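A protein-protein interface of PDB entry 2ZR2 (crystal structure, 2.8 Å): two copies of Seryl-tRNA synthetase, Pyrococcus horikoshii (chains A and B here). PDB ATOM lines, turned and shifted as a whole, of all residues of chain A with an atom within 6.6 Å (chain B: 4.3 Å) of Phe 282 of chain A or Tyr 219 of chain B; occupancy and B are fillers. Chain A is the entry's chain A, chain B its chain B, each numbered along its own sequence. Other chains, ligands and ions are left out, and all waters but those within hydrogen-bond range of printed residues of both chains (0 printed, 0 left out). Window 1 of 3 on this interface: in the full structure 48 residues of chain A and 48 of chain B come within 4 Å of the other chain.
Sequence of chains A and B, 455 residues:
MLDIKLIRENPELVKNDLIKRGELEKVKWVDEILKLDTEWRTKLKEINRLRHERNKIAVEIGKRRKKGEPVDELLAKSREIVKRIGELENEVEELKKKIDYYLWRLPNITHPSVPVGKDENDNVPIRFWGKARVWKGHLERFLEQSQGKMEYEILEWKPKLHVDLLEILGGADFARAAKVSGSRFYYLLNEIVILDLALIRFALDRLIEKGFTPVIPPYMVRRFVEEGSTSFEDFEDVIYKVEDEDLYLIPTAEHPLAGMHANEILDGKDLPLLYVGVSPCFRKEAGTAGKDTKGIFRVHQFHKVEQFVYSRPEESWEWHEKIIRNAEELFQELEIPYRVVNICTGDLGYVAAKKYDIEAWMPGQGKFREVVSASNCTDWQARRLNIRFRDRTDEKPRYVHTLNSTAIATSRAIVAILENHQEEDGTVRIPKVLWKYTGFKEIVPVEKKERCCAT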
ATOM      1  N   SER A 181       6.652  20.333 -19.595  1.00  0.00           N
ATOM      2  CA  SER A 181       5.995  19.409 -18.682  1.00  0.00           C
ATOM      3  C   SER A 181       4.900  18.528 -19.265  1.00  0.00           C
ATOM      4  O   SER A 181       4.653  17.445 -18.766  1.00  0.00           O
ATOM      5  CB  SER A 181       5.428  20.202 -17.504  1.00  0.00           C
ATOM      6  OG  SER A 181       6.462  20.899 -16.831  1.00  0.00           O
ATOM      7  N   PHE A 185      -0.391  21.708 -17.719  1.00  0.00           N
ATOM      8  CA  PHE A 185       0.591  22.395 -16.873  1.00  0.00           C
ATOM      9  C   PHE A 185       0.677  23.786 -17.519  1.00  0.00           C
ATOM     10  O   PHE A 185       0.219  23.965 -18.635  1.00  0.00           O
ATOM     11  CB  PHE A 185       1.971  21.749 -16.940  1.00  0.00           C
ATOM     12  CG  PHE A 185       2.163  20.629 -15.983  1.00  0.00           C
ATOM     13  CD1 PHE A 185       2.079  19.316 -16.409  1.00  0.00           C
ATOM     14  CD2 PHE A 185       2.429  20.889 -14.645  1.00  0.00           C
ATOM     15  CE1 PHE A 185       2.256  18.270 -15.508  1.00  0.00           C
ATOM     16  CE2 PHE A 185       2.610  19.856 -13.730  1.00  0.00           C
ATOM     17  CZ  PHE A 185       2.525  18.538 -14.161  1.00  0.00           C
ATOM     18  N   TYR A 186       1.281  24.760 -16.855  1.00  0.00           N
ATOM     19  CA  TYR A 186       1.359  26.092 -17.445  1.00  0.00           C
ATOM     20  C   TYR A 186       2.405  26.968 -16.775  1.00  0.00           C
ATOM     21  O   TYR A 186       2.913  26.630 -15.708  1.00  0.00           O
ATOM     22  CB  TYR A 186       0.029  26.783 -17.261  1.00  0.00           C
ATOM     23  CG  TYR A 186      -0.385  26.766 -15.809  1.00  0.00           C
ATOM     24  CD1 TYR A 186      -1.175  25.729 -15.308  1.00  0.00           C
ATOM     25  CD2 TYR A 186       0.096  27.724 -14.907  1.00  0.00           C
ATOM     26  CE1 TYR A 186      -1.476  25.643 -13.945  1.00  0.00           C
ATOM     27  CE2 TYR A 186      -0.194  27.646 -13.536  1.00  0.00           C
ATOM     28  CZ  TYR A 186      -0.984  26.599 -13.069  1.00  0.00           C
ATOM     29  OH  TYR A 186      -1.303  26.496 -11.734  1.00  0.00           O
ATOM     30  N   TYR A 219       4.466  19.327   1.488  1.00  0.00           N
ATOM     31  CA  TYR A 219       3.786  19.143   0.219  1.00  0.00           C
ATOM     32  C   TYR A 219       3.840  17.663  -0.188  1.00  0.00           C
ATOM     33  O   TYR A 219       3.125  17.233  -1.085  1.00  0.00           O
ATOM     34  CB  TYR A 219       4.447  20.048  -0.825  1.00  0.00           C
ATOM     35  CG  TYR A 219       4.387  21.524  -0.459  1.00  0.00           C
ATOM     36  CD1 TYR A 219       5.299  22.428  -0.994  1.00  0.00           C
ATOM     37  CD2 TYR A 219       3.410  22.018   0.416  1.00  0.00           C
ATOM     38  CE1 TYR A 219       5.251  23.779  -0.674  1.00  0.00           C
ATOM     39  CE2 TYR A 219       3.351  23.366   0.742  1.00  0.00           C
ATOM     40  CZ  TYR A 219       4.280  24.246   0.192  1.00  0.00           C
ATOM     41  OH  TYR A 219       4.263  25.588   0.513  1.00  0.00           O
ATOM     42  N   VAL A 238      -6.013  10.382  -8.703  1.00  0.00           N
ATOM     43  CA  VAL A 238      -5.529  11.710  -8.413  1.00  0.00           C
ATOM     44  C   VAL A 238      -4.148  11.886  -7.799  1.00  0.00           C
ATOM     45  O   VAL A 238      -3.442  12.836  -8.132  1.00  0.00           O
ATOM     46  CB  VAL A 238      -6.595  12.483  -7.550  1.00  0.00           C
ATOM     47  CG1 VAL A 238      -7.835  11.656  -7.369  1.00  0.00           C
ATOM     48  CG2 VAL A 238      -6.049  12.837  -6.223  1.00  0.00           C
ATOM     49  N   ILE A 239      -3.739  10.969  -6.940  1.00  0.00           N
ATOM     50  CA  ILE A 239      -2.466  11.125  -6.261  1.00  0.00           C
ATOM     51  C   ILE A 239      -1.203  10.609  -6.939  1.00  0.00           C
ATOM     52  O   ILE A 239      -1.120   9.449  -7.339  1.00  0.00           O
ATOM     53  CB  ILE A 239      -2.563  10.507  -4.870  1.00  0.00           C
ATOM     54  CG1 ILE A 239      -3.729  11.145  -4.115  1.00  0.00           C
ATOM     55  CG2 ILE A 239      -1.274  10.722  -4.116  1.00  0.00           C
ATOM     56  CD1 ILE A 239      -4.154  10.343  -2.907  1.00  0.00           C
ATOM     57  N   TYR A 240      -0.218  11.498  -7.037  1.00  0.00           N
ATOM     58  CA  TYR A 240       1.095  11.204  -7.618  1.00  0.00           C
ATOM     59  C   TYR A 240       2.008  10.641  -6.539  1.00  0.00           C
ATOM     60  O   TYR A 240       2.123  11.215  -5.445  1.00  0.00           O
ATOM     61  CB  TYR A 240       1.802  12.468  -8.107  1.00  0.00           C
ATOM     62  CG  TYR A 240       1.306  13.079  -9.376  1.00  0.00           C
ATOM     63  CD1 TYR A 240       1.500  12.448 -10.595  1.00  0.00           C
ATOM     64  CD2 TYR A 240       0.709  14.332  -9.372  1.00  0.00           C
ATOM     65  CE1 TYR A 240       1.121  13.056 -11.784  1.00  0.00           C
ATOM     66  CE2 TYR A 240       0.324  14.947 -10.555  1.00  0.00           C
ATOM     67  CZ  TYR A 240       0.530  14.307 -11.753  1.00  0.00           C
ATOM     68  OH  TYR A 240       0.123  14.896 -12.920  1.00  0.00           O
ATOM     69  N   LEU A 249       2.613  13.289  -3.353  1.00  0.00           N
ATOM     70  CA  LEU A 249       2.393  14.729  -3.500  1.00  0.00           C
ATOM     71  C   LEU A 249       0.966  15.000  -3.047  1.00  0.00           C
ATOM     72  O   LEU A 249       0.021  14.370  -3.521  1.00  0.00           O
ATOM     73  CB  LEU A 249       2.580  15.162  -4.957  1.00  0.00           C
ATOM     74  CG  LEU A 249       3.985  15.028  -5.565  1.00  0.00           C
ATOM     75  CD1 LEU A 249       3.937  15.393  -7.033  1.00  0.00           C
ATOM     76  CD2 LEU A 249       4.955  15.936  -4.849  1.00  0.00           C
ATOM     77  N   ILE A 250       0.799  15.928  -2.118  1.00  0.00           N
ATOM     78  CA  ILE A 250      -0.528  16.214  -1.615  1.00  0.00           C
ATOM     79  C   ILE A 250      -1.404  16.883  -2.664  1.00  0.00           C
ATOM     80  O   ILE A 250      -0.957  17.774  -3.386  1.00  0.00           O
ATOM     81  CB  ILE A 250      -0.464  17.115  -0.373  1.00  0.00           C
ATOM     82  CG1 ILE A 250       0.243  18.424  -0.714  1.00  0.00           C
ATOM     83  CG2 ILE A 250       0.280  16.408   0.752  1.00  0.00           C
ATOM     84  CD1 ILE A 250       0.086  19.445   0.361  1.00  0.00           C
ATOM     85  N   PRO A 251      -2.664  16.440  -2.775  1.00  0.00           N
ATOM     86  CA  PRO A 251      -3.625  16.996  -3.735  1.00  0.00           C
ATOM     87  C   PRO A 251      -4.370  18.183  -3.144  1.00  0.00           C
ATOM     88  O   PRO A 251      -5.119  18.873  -3.838  1.00  0.00           O
ATOM     89  CB  PRO A 251      -4.551  15.826  -4.002  1.00  0.00           C
ATOM     90  CG  PRO A 251      -4.566  15.124  -2.676  1.00  0.00           C
ATOM     91  CD  PRO A 251      -3.125  15.133  -2.270  1.00  0.00           C
ATOM     92  N   THR A 252      -4.134  18.412  -1.856  1.00  0.00           N
ATOM     93  CA  THR A 252      -4.767  19.489  -1.103  1.00  0.00           C
ATOM     94  C   THR A 252      -4.142  19.542   0.296  1.00  0.00           C
ATOM     95  O   THR A 252      -3.739  18.519   0.831  1.00  0.00           O
ATOM     96  CB  THR A 252      -6.290  19.237  -0.985  1.00  0.00           C
ATOM     97  OG1 THR A 252      -6.823  20.021   0.085  1.00  0.00           O
ATOM     98  CG2 THR A 252      -6.579  17.759  -0.739  1.00  0.00           C
ATOM     99  N   SER A 279      -0.893  25.781   0.182  1.00  0.00           N
ATOM    100  CA  SER A 279      -0.002  24.793  -0.395  1.00  0.00           C
ATOM    101  C   SER A 279      -0.260  24.568  -1.854  1.00  0.00           C
ATOM    102  O   SER A 279      -1.355  24.812  -2.333  1.00  0.00           O
ATOM    103  CB  SER A 279      -0.166  23.442   0.296  1.00  0.00           C
ATOM    104  OG  SER A 279      -1.159  22.678  -0.362  1.00  0.00           O
ATOM    105  N   PRO A 280       0.774  24.163  -2.600  1.00  0.00           N
ATOM    106  CA  PRO A 280       0.463  23.921  -4.008  1.00  0.00           C
ATOM    107  C   PRO A 280      -0.316  22.597  -3.940  1.00  0.00           C
ATOM    108  O   PRO A 280      -0.251  21.884  -2.929  1.00  0.00           O
ATOM    109  CB  PRO A 280       1.843  23.767  -4.655  1.00  0.00           C
ATOM    110  CG  PRO A 280       2.755  23.379  -3.496  1.00  0.00           C
ATOM    111  CD  PRO A 280       2.231  24.223  -2.371  1.00  0.00           C
ATOM    112  N   CYS A 281      -1.071  22.275  -4.979  1.00  0.00           N
ATOM    113  CA  CYS A 281      -1.828  21.035  -4.990  1.00  0.00           C
ATOM    114  C   CYS A 281      -1.478  20.314  -6.267  1.00  0.00           C
ATOM    115  O   CYS A 281      -1.353  20.946  -7.311  1.00  0.00           O
ATOM    116  CB  CYS A 281      -3.330  21.320  -4.935  1.00  0.00           C
ATOM    117  SG  CYS A 281      -3.864  22.152  -3.420  1.00  0.00           S
ATOM    118  N   PHE A 282      -1.325  18.994  -6.180  1.00  0.00           N
ATOM    119  CA  PHE A 282      -0.964  18.186  -7.340  1.00  0.00           C
ATOM    120  C   PHE A 282      -2.006  17.115  -7.602  1.00  0.00           C
ATOM    121  O   PHE A 282      -2.330  16.329  -6.718  1.00  0.00           O
ATOM    122  CB  PHE A 282       0.421  17.552  -7.124  1.00  0.00           C
ATOM    123  CG  PHE A 282       1.503  18.558  -6.825  1.00  0.00           C
ATOM    124  CD1 PHE A 282       1.718  19.007  -5.526  1.00  0.00           C
ATOM    125  CD2 PHE A 282       2.270  19.100  -7.848  1.00  0.00           C
ATOM    126  CE1 PHE A 282       2.673  19.982  -5.252  1.00  0.00           C
ATOM    127  CE2 PHE A 282       3.232  20.081  -7.582  1.00  0.00           C
ATOM    128  CZ  PHE A 282       3.433  20.522  -6.282  1.00  0.00           C
ATOM    129  N   ARG A 283      -2.521  17.083  -8.827  1.00  0.00           N
ATOM    130  CA  ARG A 283      -3.550  16.111  -9.200  1.00  0.00           C
ATOM    131  C   ARG A 283      -3.278  15.537 -10.577  1.00  0.00           C
ATOM    132  O   ARG A 283      -2.942  16.264 -11.512  1.00  0.00           O
ATOM    133  CB  ARG A 283      -4.933  16.768  -9.224  1.00  0.00           C
ATOM    134  CG  ARG A 283      -5.049  18.006  -8.364  1.00  0.00           C
ATOM    135  CD  ARG A 283      -5.678  17.752  -7.019  1.00  0.00           C
ATOM    136  NE  ARG A 283      -7.115  17.574  -7.157  1.00  0.00           N
ATOM    137  CZ  ARG A 283      -8.018  18.085  -6.324  1.00  0.00           C
ATOM    138  NH1 ARG A 283      -7.641  18.819  -5.282  1.00  0.00           N
ATOM    139  NH2 ARG A 283      -9.305  17.849  -6.537  1.00  0.00           N
ATOM    140  N   LYS A 284      -3.438  14.224 -10.697  1.00  0.00           N
ATOM    141  CA  LYS A 284      -3.224  13.539 -11.961  1.00  0.00           C
ATOM    142  C   LYS A 284      -4.345  13.895 -12.922  1.00  0.00           C
ATOM    143  O   LYS A 284      -4.116  14.027 -14.117  1.00  0.00           O
ATOM    144  CB  LYS A 284      -3.226  12.023 -11.766  1.00  0.00           C
ATOM    145  CG  LYS A 284      -2.003  11.432 -11.088  1.00  0.00           C
ATOM    146  CD  LYS A 284      -2.184   9.921 -10.885  1.00  0.00           C
ATOM    147  CE  LYS A 284      -0.983   9.271 -10.201  1.00  0.00           C
ATOM    148  NZ  LYS A 284      -1.219   7.835  -9.859  1.00  0.00           N
ATOM    149  N   VAL A 299      -6.156  21.862 -14.008  1.00  0.00           N
ATOM    150  CA  VAL A 299      -4.763  21.576 -14.315  1.00  0.00           C
ATOM    151  C   VAL A 299      -4.128  20.611 -13.330  1.00  0.00           C
ATOM    152  O   VAL A 299      -4.751  20.191 -12.365  1.00  0.00           O
ATOM    153  CB  VAL A 299      -3.960  22.885 -14.299  1.00  0.00           C
ATOM    154  CG1 VAL A 299      -4.379  23.772 -15.448  1.00  0.00           C
ATOM    155  CG2 VAL A 299      -4.231  23.622 -12.992  1.00  0.00           C
ATOM    156  N   HIS A 300      -2.870  20.273 -13.574  1.00  0.00           N
ATOM    157  CA  HIS A 300      -2.153  19.374 -12.687  1.00  0.00           C
ATOM    158  C   HIS A 300      -1.677  20.029 -11.386  1.00  0.00           C
ATOM    159  O   HIS A 300      -1.558  19.336 -10.368  1.00  0.00           O
ATOM    160  CB  HIS A 300      -0.973  18.750 -13.423  1.00  0.00           C
ATOM    161  CG  HIS A 300      -1.389  17.773 -14.470  1.00  0.00           C
ATOM    162  ND1 HIS A 300      -2.163  16.668 -14.185  1.00  0.00           N
ATOM    163  CD2 HIS A 300      -1.155  17.735 -15.800  1.00  0.00           C
ATOM    164  CE1 HIS A 300      -2.382  15.991 -15.295  1.00  0.00           C
ATOM    165  NE2 HIS A 300      -1.782  16.616 -16.289  1.00  0.00           N
ATOM    166  N   GLN A 301      -1.389  21.338 -11.411  1.00  0.00           N
ATOM    167  CA  GLN A 301      -0.972  22.029 -10.191  1.00  0.00           C
ATOM    168  C   GLN A 301      -1.686  23.362  -9.985  1.00  0.00           C
ATOM    169  O   GLN A 301      -1.921  24.109 -10.931  1.00  0.00           O
ATOM    170  CB  GLN A 301       0.551  22.270 -10.163  1.00  0.00           C
ATOM    171  CG  GLN A 301       1.001  23.504 -10.897  1.00  0.00           C
ATOM    172  CD  GLN A 301       2.506  23.663 -10.926  1.00  0.00           C
ATOM    173  OE1 GLN A 301       3.232  22.703 -11.180  1.00  0.00           O
ATOM    174  NE2 GLN A 301       2.984  24.881 -10.699  1.00  0.00           N
ATOM    175  N   PHE A 302      -2.041  23.643  -8.736  1.00  0.00           N
ATOM    176  CA  PHE A 302      -2.677  24.910  -8.390  1.00  0.00           C
ATOM    177  C   PHE A 302      -2.449  25.200  -6.924  1.00  0.00           C
ATOM    178  O   PHE A 302      -2.138  24.304  -6.148  1.00  0.00           O
ATOM    179  CB  PHE A 302      -4.181  24.914  -8.677  1.00  0.00           C
ATOM    180  CG  PHE A 302      -4.932  23.779  -8.046  1.00  0.00           C
ATOM    181  CD1 PHE A 302      -4.856  22.496  -8.576  1.00  0.00           C
ATOM    182  CD2 PHE A 302      -5.730  23.992  -6.925  1.00  0.00           C
ATOM    183  CE1 PHE A 302      -5.569  21.434  -7.993  1.00  0.00           C
ATOM    184  CE2 PHE A 302      -6.448  22.935  -6.333  1.00  0.00           C
ATOM    185  CZ  PHE A 302      -6.364  21.656  -6.872  1.00  0.00           C
ATOM    186  N   HIS A 303      -2.593  26.466  -6.565  1.00  0.00           N
ATOM    187  CA  HIS A 303      -2.422  26.918  -5.196  1.00  0.00           C
ATOM    188  C   HIS A 303      -3.779  26.983  -4.527  1.00  0.00           C
ATOM    189  O   HIS A 303      -4.775  27.357  -5.153  1.00  0.00           O
ATOM    190  CB  HIS A 303      -1.782  28.283  -5.221  1.00  0.00           C
ATOM    191  CG  HIS A 303      -0.418  28.281  -5.816  1.00  0.00           C
ATOM    192  ND1 HIS A 303       0.161  29.406  -6.360  1.00  0.00           N
ATOM    193  CD2 HIS A 303       0.501  27.290  -5.928  1.00  0.00           C
ATOM    194  CE1 HIS A 303       1.379  29.110  -6.784  1.00  0.00           C
ATOM    195  NE2 HIS A 303       1.608  27.830  -6.534  1.00  0.00           N
ATOM    196  N   ILE B 216       5.449  32.033 -12.588  1.00  0.00           N
ATOM    197  CA  ILE B 216       5.155  30.890 -11.750  1.00  0.00           C
ATOM    198  C   ILE B 216       5.215  29.764 -12.767  1.00  0.00           C
ATOM    199  O   ILE B 216       4.375  29.676 -13.661  1.00  0.00           O
ATOM    200  CB  ILE B 216       3.753  30.972 -11.124  1.00  0.00           C
ATOM    201  CG1 ILE B 216       3.708  32.127 -10.114  1.00  0.00           C
ATOM    202  CG2 ILE B 216       3.416  29.640 -10.467  1.00  0.00           C
ATOM    203  CD1 ILE B 216       2.432  32.237  -9.319  1.00  0.00           C
ATOM    204  N   PRO B 217       6.223  28.896 -12.659  1.00  0.00           N
ATOM    205  CA  PRO B 217       6.401  27.778 -13.586  1.00  0.00           C
ATOM    206  C   PRO B 217       5.816  26.464 -13.122  1.00  0.00           C
ATOM    207  O   PRO B 217       5.162  26.368 -12.075  1.00  0.00           O
ATOM    208  CB  PRO B 217       7.909  27.662 -13.657  1.00  0.00           C
ATOM    209  CG  PRO B 217       8.252  27.799 -12.179  1.00  0.00           C
ATOM    210  CD  PRO B 217       7.366  28.974 -11.729  1.00  0.00           C
ATOM    211  N   PRO B 218       6.040  25.422 -13.924  1.00  0.00           N
ATOM    212  CA  PRO B 218       5.547  24.091 -13.573  1.00  0.00           C
ATOM    213  C   PRO B 218       6.463  23.595 -12.468  1.00  0.00           C
ATOM    214  O   PRO B 218       7.670  23.870 -12.499  1.00  0.00           O
ATOM    215  CB  PRO B 218       5.730  23.315 -14.861  1.00  0.00           C
ATOM    216  CG  PRO B 218       5.469  24.367 -15.896  1.00  0.00           C
ATOM    217  CD  PRO B 218       6.268  25.527 -15.374  1.00  0.00           C
ATOM    218  N   TYR B 219       5.903  22.888 -11.492  1.00  0.00           N
ATOM    219  CA  TYR B 219       6.711  22.374 -10.398  1.00  0.00           C
ATOM    220  C   TYR B 219       7.266  20.997 -10.735  1.00  0.00           C
ATOM    221  O   TYR B 219       8.136  20.477 -10.031  1.00  0.00           O
ATOM    222  CB  TYR B 219       5.878  22.336  -9.117  1.00  0.00           C
ATOM    223  CG  TYR B 219       5.356  23.705  -8.725  1.00  0.00           C
ATOM    224  CD1 TYR B 219       4.310  23.837  -7.825  1.00  0.00           C
ATOM    225  CD2 TYR B 219       5.905  24.867  -9.266  1.00  0.00           C
ATOM    226  CE1 TYR B 219       3.816  25.096  -7.474  1.00  0.00           C
ATOM    227  CE2 TYR B 219       5.425  26.121  -8.920  1.00  0.00           C
ATOM    228  CZ  TYR B 219       4.376  26.229  -8.028  1.00  0.00           C
ATOM    229  OH  TYR B 219       3.862  27.464  -7.707  1.00  0.00           O
ATOM    230  N   MET B 220       6.765  20.433 -11.835  1.00  0.00           N
ATOM    231  CA  MET B 220       7.168  19.115 -12.355  1.00  0.00           C
ATOM    232  C   MET B 220       7.558  19.283 -13.814  1.00  0.00           C
ATOM    233  O   MET B 220       6.836  19.916 -14.587  1.00  0.00           O
ATOM    234  CB  MET B 220       6.008  18.115 -12.279  1.00  0.00           C
ATOM    235  CG  MET B 220       5.482  17.854 -10.871  1.00  0.00           C
ATOM    236  SD  MET B 220       3.953  16.939 -10.870  1.00  0.00           S
ATOM    237  CE  MET B 220       4.570  15.307 -10.841  1.00  0.00           C
ATOM    238  N   TYR B 248       9.487  15.142 -13.145  1.00  0.00           N
ATOM    239  CA  TYR B 248      10.424  15.346 -12.065  1.00  0.00           C
ATOM    240  C   TYR B 248      10.107  16.608 -11.288  1.00  0.00           C
ATOM    241  O   TYR B 248       9.892  17.664 -11.870  1.00  0.00           O
ATOM    242  CB  TYR B 248      11.815  15.432 -12.641  1.00  0.00           C
ATOM    243  CG  TYR B 248      12.204  14.194 -13.389  1.00  0.00           C
ATOM    244  CD1 TYR B 248      11.675  13.928 -14.659  1.00  0.00           C
ATOM    245  CD2 TYR B 248      13.096  13.275 -12.830  1.00  0.00           C
ATOM    246  CE1 TYR B 248      12.022  12.778 -15.354  1.00  0.00           C
ATOM    247  CE2 TYR B 248      13.457  12.121 -13.517  1.00  0.00           C
ATOM    248  CZ  TYR B 248      12.919  11.878 -14.773  1.00  0.00           C
ATOM    249  OH  TYR B 248      13.281  10.745 -15.453  1.00  0.00           O
ATOM    250  N   LEU B 249      10.048  16.477  -9.968  1.00  0.00           N
ATOM    251  CA  LEU B 249       9.776  17.601  -9.089  1.00  0.00           C
ATOM    252  C   LEU B 249      10.965  18.529  -9.213  1.00  0.00           C
ATOM    253  O   LEU B 249      12.104  18.084  -9.092  1.00  0.00           O
ATOM    254  CB  LEU B 249       9.627  17.106  -7.651  1.00  0.00           C
ATOM    255  CG  LEU B 249       8.322  16.357  -7.376  1.00  0.00           C
ATOM    256  CD1 LEU B 249       8.243  15.913  -5.926  1.00  0.00           C
ATOM    257  CD2 LEU B 249       7.174  17.303  -7.660  1.00  0.00           C
ATOM    258  N   ILE B 250      10.712  19.811  -9.456  1.00  0.00           N
ATOM    259  CA  ILE B 250      11.805  20.760  -9.621  1.00  0.00           C
ATOM    260  C   ILE B 250      12.497  21.184  -8.314  1.00  0.00           C
ATOM    261  O   ILE B 250      11.849  21.458  -7.308  1.00  0.00           O
ATOM    262  CB  ILE B 250      11.335  22.062 -10.352  1.00  0.00           C
ATOM    263  CG1 ILE B 250      10.373  22.852  -9.462  1.00  0.00           C
ATOM    264  CG2 ILE B 250      10.674  21.726 -11.667  1.00  0.00           C
ATOM    265  CD1 ILE B 250      10.276  24.291  -9.838  1.00  0.00           C
ATOM    266  N   SER B 279       8.591  29.655  -6.695  1.00  0.00           N
ATOM    267  CA  SER B 279       8.123  28.278  -6.664  1.00  0.00           C
ATOM    268  C   SER B 279       8.619  27.482  -5.477  1.00  0.00           C
ATOM    269  O   SER B 279       9.540  27.887  -4.766  1.00  0.00           O
ATOM    270  CB  SER B 279       8.550  27.532  -7.923  1.00  0.00           C
ATOM    271  OG  SER B 279       9.779  26.863  -7.709  1.00  0.00           O
ATOM    272  N   PRO B 280       7.961  26.356  -5.205  1.00  0.00           N
ATOM    273  CA  PRO B 280       8.462  25.581  -4.082  1.00  0.00           C
ATOM    274  C   PRO B 280       9.623  24.806  -4.717  1.00  0.00           C
ATOM    275  O   PRO B 280       9.718  24.733  -5.944  1.00  0.00           O
ATOM    276  CB  PRO B 280       7.277  24.695  -3.712  1.00  0.00           C
ATOM    277  CG  PRO B 280       6.551  24.540  -5.022  1.00  0.00           C
ATOM    278  CD  PRO B 280       6.608  25.920  -5.590  1.00  0.00           C
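The side-chain amide nitrogen of Gln 301 of chain A sits at hydrogen-bond distance from the backbone carbonyl oxygen of Pro 217 of chain B (3.0 Å). The side-chain amide oxygen (OE1) of Gln 301 of chain A is in hydrogen-bond range of the backbone NH (N) of Tyr 219 of chain B (2.7 Å). The side-chain hydroxyl (OH) of Tyr 219 of chain B is in hydrogen-bond range of a ring nitrogen (NE2) of His 303 of chain A, 2.6 Å away. The backbone carbonyl oxygen (O) of Met 220 of chain B lies within hydrogen-bond range of the side-chain hydroxyl (OG) of Ser 181 of chain A, 2.5 Å away.
Among the printed residues, pairs that only touch across the chains: Ser 181 of chain A with Pro 218 of chain B, Tyr 186 of chain A with Pro 218 of chain B, Leu 249 of chain A with Leu 249 of chain B, Gln 301 of chain A with Pro 218 of chain B, Pro 280 of chain A with Tyr 219 of chain B, Phe 282 of chain A with Tyr 219 of chain B, Tyr 219 of chain A with Pro 280 of chain B, Leu 249 of chain A with Met 220 of chain B, Tyr 186 of chain A with Pro 217 of chain B, Phe 185 of chain A with Met 220 of chain B and Tyr 186 of chain A with Ile 216 of chain B.
Tyr 219 of chain A touches Pro 280 of chain B, and with the chains exchanged Pro 280 of chain A touches Tyr 219 of chain B. Leu 249 of chain A touches its own counterpart, Leu 249 of chain B. 5 positions are printed for both chains. Of the 15 pairs that touch across the chains among the printed residues, 3 have their exchanged pair printed and touching as well.
O of Tyr 240 of chain A sits at hydrogen-bond distance from N of Leu 249 of chain A (3.0 Å). The backbone carbonyl oxygen (O) of Tyr 219 of chain B sits at hydrogen-bond distance from the backbone NH (N) of Ile 250 of chain B. The backbone NH of Phe 282 of chain A is in hydrogen-bond range of the backbone carbonyl oxygen of Ile 250 of chain A, 3.1 Å away. The backbone carbonyl oxygen of Gln 301 of chain A is in hydrogen-bond range of the side-chain hydroxyl of Tyr 186 of chain A (2.6 Å). The backbone carbonyl oxygen (O) of Tyr 219 of chain A is in hydrogen-bond range of the backbone NH (N) of Ile 250 of chain A, at 2.9 Å.
Of the 22 printed residues of chain A, 9 touch a printed residue of chain B. Hydrophobic or aromatic side chains of chain A within 4 Å of the printed part of chain B: Phe 185, Tyr 219, Leu 249, Pro 280, Phe 282 and His 303. Hydrophobic or aromatic side chains of chain B that line the printed part of chain A: Pro 218, Tyr 219, Met 220, Leu 249 and Pro 280. Among the printed residues, 15 pairs touch across the chains. Among the printed residues, no Asp or Glu carboxylate lies within 4 Å of a Lys or Arg side-chain nitrogen of the other chain.
Phe 282 of chain A touches just one residue of chain B: Tyr 219 (3.8 Å). Tyr 219 of chain B touches four residues of chain A. Of the printed residues of chain B, Ser 181 of chain A touches Pro 218 and Met 220. Of the printed residues of chain A, Pro 217 of chain B touches Tyr 186 and Gln 301. Lys 284 of chain A touches none of the printed residues of chain B. The nearest residue of chain A that does not touch Tyr 219 of chain B is Phe 185 of chain A (5.0 Å).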
